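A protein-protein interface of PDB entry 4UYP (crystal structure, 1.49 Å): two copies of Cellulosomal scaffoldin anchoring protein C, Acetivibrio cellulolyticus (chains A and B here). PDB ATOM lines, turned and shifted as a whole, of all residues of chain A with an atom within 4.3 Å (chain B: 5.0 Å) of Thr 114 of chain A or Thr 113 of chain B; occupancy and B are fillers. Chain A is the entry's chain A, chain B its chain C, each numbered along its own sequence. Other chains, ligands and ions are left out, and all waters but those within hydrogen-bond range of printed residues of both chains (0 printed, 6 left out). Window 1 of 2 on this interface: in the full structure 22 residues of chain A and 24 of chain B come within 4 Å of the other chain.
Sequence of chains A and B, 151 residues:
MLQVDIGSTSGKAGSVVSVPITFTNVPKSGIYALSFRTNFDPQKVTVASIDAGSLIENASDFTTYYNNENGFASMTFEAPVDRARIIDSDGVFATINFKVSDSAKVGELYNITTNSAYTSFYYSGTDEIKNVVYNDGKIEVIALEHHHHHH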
ATOM      1  N   ILE A   6      38.856  16.933 -27.194  1.00  0.00           N
ATOM      2  CA  ILE A   6      39.004  15.746 -26.323  1.00  0.00           C
ATOM      3  C   ILE A   6      39.139  14.575 -27.269  1.00  0.00           C
ATOM      4  O   ILE A   6      38.193  14.307 -28.088  1.00  0.00           O
ATOM      5  CB  ILE A   6      37.749  15.599 -25.464  1.00  0.00           C
ATOM      6  CG1 ILE A   6      37.543  16.809 -24.545  1.00  0.00           C
ATOM      7  CG2 ILE A   6      37.856  14.232 -24.710  1.00  0.00           C
ATOM      8  CD1 ILE A   6      36.260  16.670 -23.696  1.00  0.00           C
ATOM      9  N   PHE A  36      39.491  23.792 -17.540  1.00  0.00           N
ATOM     10  CA  PHE A  36      38.864  22.860 -18.469  1.00  0.00           C
ATOM     11  C   PHE A  36      38.247  21.751 -17.640  1.00  0.00           C
ATOM     12  O   PHE A  36      38.948  21.101 -16.851  1.00  0.00           O
ATOM     13  CB  PHE A  36      39.915  22.255 -19.373  1.00  0.00           C
ATOM     14  CG  PHE A  36      39.333  21.378 -20.444  1.00  0.00           C
ATOM     15  CD1 PHE A  36      38.801  22.011 -21.551  1.00  0.00           C
ATOM     16  CD2 PHE A  36      39.383  19.973 -20.358  1.00  0.00           C
ATOM     17  CE1 PHE A  36      38.205  21.312 -22.582  1.00  0.00           C
ATOM     18  CE2 PHE A  36      38.760  19.238 -21.447  1.00  0.00           C
ATOM     19  CZ  PHE A  36      38.176  19.949 -22.473  1.00  0.00           C
ATOM     20  N   ARG A  37      36.960  21.462 -17.843  1.00  0.00           N
ATOM     21  CA  ARG A  37      36.220  20.391 -17.100  1.00  0.00           C
ATOM     22  C   ARG A  37      35.581  19.472 -18.093  1.00  0.00           C
ATOM     23  O   ARG A  37      34.919  19.904 -19.060  1.00  0.00           O
ATOM     24  CB  ARG A  37      35.148  20.966 -16.157  1.00  0.00           C
ATOM     25  CG  ARG A  37      34.488  19.830 -15.436  1.00  0.00           C
ATOM     26  CD  ARG A  37      33.479  20.243 -14.377  1.00  0.00           C
ATOM     27  NE  ARG A  37      34.148  20.962 -13.306  1.00  0.00           N
ATOM     28  CZ  ARG A  37      33.563  21.242 -12.154  1.00  0.00           C
ATOM     29  NH1 ARG A  37      32.289  20.863 -11.885  1.00  0.00           N
ATOM     30  NH2 ARG A  37      34.234  22.011 -11.223  1.00  0.00           N
ATOM     31  N   THR A 113      32.776  14.629 -22.254  1.00  0.00           N
ATOM     32  CA  THR A 113      32.181  15.869 -22.732  1.00  0.00           C
ATOM     33  C   THR A 113      32.838  17.083 -22.111  1.00  0.00           C
ATOM     34  O   THR A 113      33.231  17.037 -20.961  1.00  0.00           O
ATOM     35  CB  THR A 113      30.639  15.843 -22.427  1.00  0.00           C
ATOM     36  OG1 THR A 113      30.357  15.673 -21.056  1.00  0.00           O
ATOM     37  CG2 THR A 113      30.001  14.730 -23.244  1.00  0.00           C
ATOM     38  N   THR A 114      32.898  18.202 -22.818  1.00  0.00           N
ATOM     39  CA  THR A 114      33.370  19.430 -22.276  1.00  0.00           C
ATOM     40  C   THR A 114      32.321  20.189 -21.523  1.00  0.00           C
ATOM     41  O   THR A 114      31.220  20.444 -22.098  1.00  0.00           O
ATOM     42  CB  THR A 114      33.922  20.333 -23.402  1.00  0.00           C
ATOM     43  OG1 THR A 114      34.879  19.636 -24.176  1.00  0.00           O
ATOM     44  CG2 THR A 114      34.585  21.568 -22.804  1.00  0.00           C
ATOM     45  N   ASN A 115      32.530  20.647 -20.324  1.00  0.00           N
ATOM     46  CA  ASN A 115      31.540  21.327 -19.572  1.00  0.00           C
ATOM     47  C   ASN A 115      31.763  22.823 -19.753  1.00  0.00           C
ATOM     48  O   ASN A 115      32.622  23.461 -19.095  1.00  0.00           O
ATOM     49  CB  ASN A 115      31.620  20.926 -18.096  1.00  0.00           C
ATOM     50  CG  ASN A 115      30.479  21.475 -17.293  1.00  0.00           C
ATOM     51  OD1 ASN A 115      30.064  22.679 -17.451  1.00  0.00           O
ATOM     52  ND2 ASN A 115      29.956  20.679 -16.327  1.00  0.00           N
ATOM     53  N   SER A 116      30.857  23.477 -20.515  1.00  0.00           N
ATOM     54  CA  SER A 116      31.076  24.883 -20.808  1.00  0.00           C
ATOM     55  C   SER A 116      30.863  25.788 -19.616  1.00  0.00           C
ATOM     56  O   SER A 116      31.288  26.976 -19.632  1.00  0.00           O
ATOM     57  CB  SER A 116      30.310  25.332 -22.050  1.00  0.00           C
ATOM     58  OG  SER A 116      28.961  25.049 -21.752  1.00  0.00           O
ATOM     59  N   THR A 119      34.546  25.760 -17.931  1.00  0.00           N
ATOM     60  CA  THR A 119      35.651  25.828 -18.841  1.00  0.00           C
ATOM     61  C   THR A 119      35.753  27.276 -19.327  1.00  0.00           C
ATOM     62  O   THR A 119      34.742  27.821 -19.873  1.00  0.00           O
ATOM     63  CB  THR A 119      35.385  24.925 -20.020  1.00  0.00           C
ATOM     64  OG1 THR A 119      35.383  23.515 -19.472  1.00  0.00           O
ATOM     65  CG2 THR A 119      36.447  24.913 -21.093  1.00  0.00           C
ATOM     66  N   TYR A 134      34.854  24.128 -28.491  1.00  0.00           N
ATOM     67  CA  TYR A 134      35.097  22.855 -27.796  1.00  0.00           C
ATOM     68  C   TYR A 134      34.674  21.689 -28.732  1.00  0.00           C
ATOM     69  O   TYR A 134      33.559  21.755 -29.360  1.00  0.00           O
ATOM     70  CB  TYR A 134      34.372  22.811 -26.482  1.00  0.00           C
ATOM     71  CG  TYR A 134      34.595  24.008 -25.521  1.00  0.00           C
ATOM     72  CD1 TYR A 134      35.842  24.687 -25.399  1.00  0.00           C
ATOM     73  CD2 TYR A 134      33.519  24.402 -24.680  1.00  0.00           C
ATOM     74  CE1 TYR A 134      35.944  25.837 -24.594  1.00  0.00           C
ATOM     75  CE2 TYR A 134      33.596  25.387 -23.769  1.00  0.00           C
ATOM     76  CZ  TYR A 134      34.738  26.171 -23.775  1.00  0.00           C
ATOM     77  OH  TYR A 134      34.916  27.296 -22.905  1.00  0.00           O
ATOM     78  N   ASP A 136      34.223  17.361 -28.482  1.00  0.00           N
ATOM     79  CA  ASP A 136      34.242  16.255 -27.469  1.00  0.00           C
ATOM     80  C   ASP A 136      34.711  14.982 -28.009  1.00  0.00           C
ATOM     81  O   ASP A 136      34.954  14.797 -29.236  1.00  0.00           O
ATOM     82  CB  ASP A 136      32.847  16.197 -26.880  1.00  0.00           C
ATOM     83  CG  ASP A 136      32.595  17.387 -25.937  1.00  0.00           C
ATOM     84  OD1 ASP A 136      33.392  18.285 -25.889  1.00  0.00           O
ATOM     85  OD2 ASP A 136      31.459  17.420 -25.430  1.00  0.00           O
ATOM     86  N   ILE B   6      22.308  19.160 -30.484  1.00  0.00           N
ATOM     87  CA  ILE B   6      22.001  20.538 -29.965  1.00  0.00           C
ATOM     88  C   ILE B   6      22.207  21.464 -31.137  1.00  0.00           C
ATOM     89  O   ILE B   6      23.367  21.575 -31.658  1.00  0.00           O
ATOM     90  CB  ILE B   6      22.885  20.879 -28.785  1.00  0.00           C
ATOM     91  CG1 ILE B   6      22.701  19.875 -27.616  1.00  0.00           C
ATOM     92  CG2 ILE B   6      22.659  22.336 -28.332  1.00  0.00           C
ATOM     93  CD1 ILE B   6      23.589  20.204 -26.461  1.00  0.00           C
ATOM     94  N   ARG B  37      21.048  16.967 -20.014  1.00  0.00           N
ATOM     95  CA  ARG B  37      21.484  18.242 -19.413  1.00  0.00           C
ATOM     96  C   ARG B  37      22.465  18.916 -20.307  1.00  0.00           C
ATOM     97  O   ARG B  37      23.355  18.265 -20.868  1.00  0.00           O
ATOM     98  CB  ARG B  37      22.174  17.894 -18.105  1.00  0.00           C
ATOM     99  CG  ARG B  37      22.643  19.213 -17.461  1.00  0.00           C
ATOM    100  CD  ARG B  37      23.275  19.061 -16.076  1.00  0.00           C
ATOM    101  NE  ARG B  37      22.306  18.533 -15.162  1.00  0.00           N
ATOM    102  CZ  ARG B  37      22.533  18.556 -13.872  1.00  0.00           C
ATOM    103  NH1 ARG B  37      23.644  19.051 -13.305  1.00  0.00           N
ATOM    104  NH2 ARG B  37      21.631  18.069 -13.020  1.00  0.00           N
ATOM    105  N   THR B  38      22.255  20.216 -20.487  1.00  0.00           N
ATOM    106  CA  THR B  38      23.176  21.105 -21.271  1.00  0.00           C
ATOM    107  C   THR B  38      23.821  22.058 -20.311  1.00  0.00           C
ATOM    108  O   THR B  38      23.166  22.638 -19.438  1.00  0.00           O
ATOM    109  CB  THR B  38      22.420  22.034 -22.290  1.00  0.00           C
ATOM    110  OG1 THR B  38      21.491  22.863 -21.626  1.00  0.00           O
ATOM    111  CG2 THR B  38      21.670  21.138 -23.351  1.00  0.00           C
ATOM    112  N   ASN B  39      25.138  22.323 -20.484  1.00  0.00           N
ATOM    113  CA  ASN B  39      25.755  23.474 -19.819  1.00  0.00           C
ATOM    114  C   ASN B  39      26.018  24.634 -20.796  1.00  0.00           C
ATOM    115  O   ASN B  39      26.082  24.444 -21.990  1.00  0.00           O
ATOM    116  CB  ASN B  39      27.125  23.013 -19.208  1.00  0.00           C
ATOM    117  CG  ASN B  39      26.892  22.028 -18.018  1.00  0.00           C
ATOM    118  OD1 ASN B  39      27.044  20.791 -18.238  1.00  0.00           O
ATOM    119  ND2 ASN B  39      26.506  22.519 -16.886  1.00  0.00           N
ATOM    120  N   PHE B  40      26.206  25.721 -20.104  1.00  0.00           N
ATOM    121  CA  PHE B  40      26.510  26.993 -20.815  1.00  0.00           C
ATOM    122  C   PHE B  40      27.177  27.928 -19.822  1.00  0.00           C
ATOM    123  O   PHE B  40      27.068  27.795 -18.601  1.00  0.00           O
ATOM    124  CB  PHE B  40      25.204  27.663 -21.337  1.00  0.00           C
ATOM    125  CG  PHE B  40      24.142  27.890 -20.249  1.00  0.00           C
ATOM    126  CD1 PHE B  40      23.189  26.818 -19.960  1.00  0.00           C
ATOM    127  CD2 PHE B  40      24.034  29.120 -19.481  1.00  0.00           C
ATOM    128  CE1 PHE B  40      22.192  27.032 -18.984  1.00  0.00           C
ATOM    129  CE2 PHE B  40      23.038  29.296 -18.526  1.00  0.00           C
ATOM    130  CZ  PHE B  40      22.112  28.233 -18.266  1.00  0.00           C
ATOM    131  N   ASN B 111      29.519  27.828 -26.423  1.00  0.00           N
ATOM    132  CA  ASN B 111      29.336  26.362 -26.572  1.00  0.00           C
ATOM    133  C   ASN B 111      28.197  25.886 -25.643  1.00  0.00           C
ATOM    134  O   ASN B 111      28.223  26.146 -24.408  1.00  0.00           O
ATOM    135  CB  ASN B 111      30.659  25.741 -26.101  1.00  0.00           C
ATOM    136  CG  ASN B 111      31.771  26.093 -27.070  1.00  0.00           C
ATOM    137  OD1 ASN B 111      31.946  25.385 -28.085  1.00  0.00           O
ATOM    138  ND2 ASN B 111      32.528  27.107 -26.737  1.00  0.00           N
ATOM    139  N   ILE B 112      27.226  25.234 -26.286  1.00  0.00           N
ATOM    140  CA  ILE B 112      26.064  24.679 -25.480  1.00  0.00           C
ATOM    141  C   ILE B 112      26.285  23.162 -25.597  1.00  0.00           C
ATOM    142  O   ILE B 112      26.200  22.550 -26.632  1.00  0.00           O
ATOM    143  CB  ILE B 112      24.744  25.124 -26.203  1.00  0.00           C
ATOM    144  CG1 ILE B 112      24.652  26.661 -26.392  1.00  0.00           C
ATOM    145  CG2 ILE B 112      23.582  24.654 -25.382  1.00  0.00           C
ATOM    146  CD1 ILE B 112      24.813  27.538 -25.137  1.00  0.00           C
ATOM    147  N   THR B 113      26.678  22.677 -24.423  1.00  0.00           N
ATOM    148  CA  THR B 113      27.317  21.348 -24.342  1.00  0.00           C
ATOM    149  C   THR B 113      26.492  20.260 -23.667  1.00  0.00           C
ATOM    150  O   THR B 113      25.940  20.540 -22.658  1.00  0.00           O
ATOM    151  CB  THR B 113      28.697  21.468 -23.524  1.00  0.00           C
ATOM    152  OG1 THR B 113      28.548  22.016 -22.253  1.00  0.00           O
ATOM    153  CG2 THR B 113      29.692  22.462 -24.312  1.00  0.00           C
ATOM    154  N   THR B 114      26.441  19.086 -24.239  1.00  0.00           N
ATOM    155  CA  THR B 114      25.765  17.910 -23.545  1.00  0.00           C
ATOM    156  C   THR B 114      26.611  17.434 -22.367  1.00  0.00           C
ATOM    157  O   THR B 114      27.827  17.179 -22.592  1.00  0.00           O
ATOM    158  CB  THR B 114      25.582  16.826 -24.527  1.00  0.00           C
ATOM    159  OG1 THR B 114      24.844  17.255 -25.695  1.00  0.00           O
ATOM    160  CG2 THR B 114      24.733  15.680 -23.841  1.00  0.00           C
ATOM    161  N   ASN B 115      26.034  17.253 -21.219  1.00  0.00           N
ATOM    162  CA  ASN B 115      26.750  16.813 -19.988  1.00  0.00           C
ATOM    163  C   ASN B 115      26.554  15.282 -19.871  1.00  0.00           C
ATOM    164  O   ASN B 115      25.475  14.858 -19.467  1.00  0.00           O
ATOM    165  CB  ASN B 115      26.296  17.611 -18.807  1.00  0.00           C
ATOM    166  CG  ASN B 115      27.142  17.362 -17.546  1.00  0.00           C
ATOM    167  OD1 ASN B 115      27.551  16.150 -17.398  1.00  0.00           O
ATOM    168  ND2 ASN B 115      27.284  18.293 -16.694  1.00  0.00           N
ATOM    169  N   ASP B 136      27.091  18.681 -30.095  1.00  0.00           N
ATOM    170  CA  ASP B 136      26.800  19.929 -29.352  1.00  0.00           C
ATOM    171  C   ASP B 136      26.581  21.107 -30.378  1.00  0.00           C
ATOM    172  O   ASP B 136      26.785  21.022 -31.580  1.00  0.00           O
ATOM    173  CB  ASP B 136      27.980  20.262 -28.440  1.00  0.00           C
ATOM    174  CG  ASP B 136      28.093  19.395 -27.205  1.00  0.00           C
ATOM    175  OD1 ASP B 136      27.116  18.627 -27.037  1.00  0.00           O
ATOM    176  OD2 ASP B 136      29.124  19.581 -26.497  1.00  0.00           O
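Of the printed residues of chain B, Thr 114 of chain A touches Thr 113 (3.1 Å). Printed residues of chain A within 4 Å of Asn 39 of chain B: Asn 115 and Ser 116. Of the printed residues of chain A, Asp 136 of chain B touches Asp 136 (3.4 Å). Printed residues of chain B within 4 Å of Ser 116 of chain A: Asn 39, Phe 40, Asn 111 and Thr 113. Of the printed residues of chain B, Asp 136 of chain A touches Asp 136. Of the printed residues of chain A, Phe 40 of chain B touches Ser 116. Phe 36 of chain A touches none of the printed residues of chain B. Arg 37 of chain A touches none of the printed residues of chain B. The nearest residue of chain B that does not touch Thr 114 of chain A is Thr 114 of chain B (4.7 Å). The nearest residue of chain A that does not touch Thr 113 of chain B is Asn 115 of chain A (4.1 Å).
The backbone carbonyl oxygen (O) of Thr 114 of chain B sits close to the side-chain hydroxyl (OG1) of Thr 113 of chain A (3.3 Å). O of Thr 114 of chain A lies close to OG1 of Thr 113 of chain B, at 3.1 Å. ND2 of Asn 115 of chain A lies within hydrogen-bond range of OD1 of Asn 39 of chain B (3.5 Å). O of Asn 39 of chain B lies within hydrogen-bond range of OG of Ser 116 of chain A, 3.0 Å away. OG of Ser 116 of chain A lies close to N of Phe 40 of chain B. OG of Ser 116 of chain A is in hydrogen-bond range of O of Asn 111 of chain B, 3.0 Å away. OG of Ser 116 of chain A sits at hydrogen-bond distance from OG1 of Thr 113 of chain B, at 3.1 Å. The backbone NH (N) of Tyr 134 of chain A is in hydrogen-bond range of the side-chain amide oxygen (OD1) of Asn 111 of chain B, at 3.2 Å. The side-chain carboxylate (OD2) of Asp 136 of chain B sits close to the side-chain carboxylate (OD2) of Asp 136 of chain A.
Printed residues of chain B that touch a printed residue of chain A: Asn 39, Phe 40, Asn 111, Thr 113, Thr 114, Asn 115 and Asp 136. Hydrophobic or aromatic side chains of chain A within 4 Å of the printed part of chain B: Tyr 134. Among the printed residues, no Asp or Glu carboxylate lies within 4 Å of a Lys or Arg side-chain nitrogen of the other chain.
Thr 113 of chain A touches Thr 114 of chain B, and with the chains exchanged Thr 114 of chain A touches Thr 113 of chain B. Thr 113 of chain A touches Asn 115 of chain B, but with the chains exchanged Asn 115 of chain A does not touch Thr 113 of chain B (4.1 Å). Asn 115 of chain A touches its own counterpart, Asn 115 of chain B. Asp 136 of chain B touches its own counterpart, Asp 136 of chain A. Positions printed for both chains: 6, 37, 113, 114, 115 and 136. Of the 11 pairs that touch across the chains among the printed residues, 4 have their exchanged pair printed and touching as well.
Thr 113 of chain A touches Asn 115 of chain B. Asn 115 of chain A touches Asn 115 of chain B (ND2 to ND2, 3.6 Å).
The backbone carbonyl oxygen of Arg 37 of chain A sits at hydrogen-bond distance from the backbone NH of Asn 115 of chain A, 2.8 Å away. The side-chain hydroxyl of Thr 119 of chain A is in hydrogen-bond range of the backbone carbonyl oxygen of Asn 115 of chain A (2.8 Å). The side-chain hydroxyl (OH) of Tyr 134 of chain A sits at hydrogen-bond distance from the backbone carbonyl oxygen (O) of Thr 119 of chain A (3.1 Å). N of Asn 115 of chain B is in hydrogen-bond range of O of Arg 37 of chain B. ND2 of Asn 115 of chain B lies within hydrogen-bond range of OD1 of Asn 39 of chain B (2.9 Å). OD1 of Asp 136 of chain B sits at hydrogen-bond distance from N of Thr 114 of chain B (2.9 Å).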
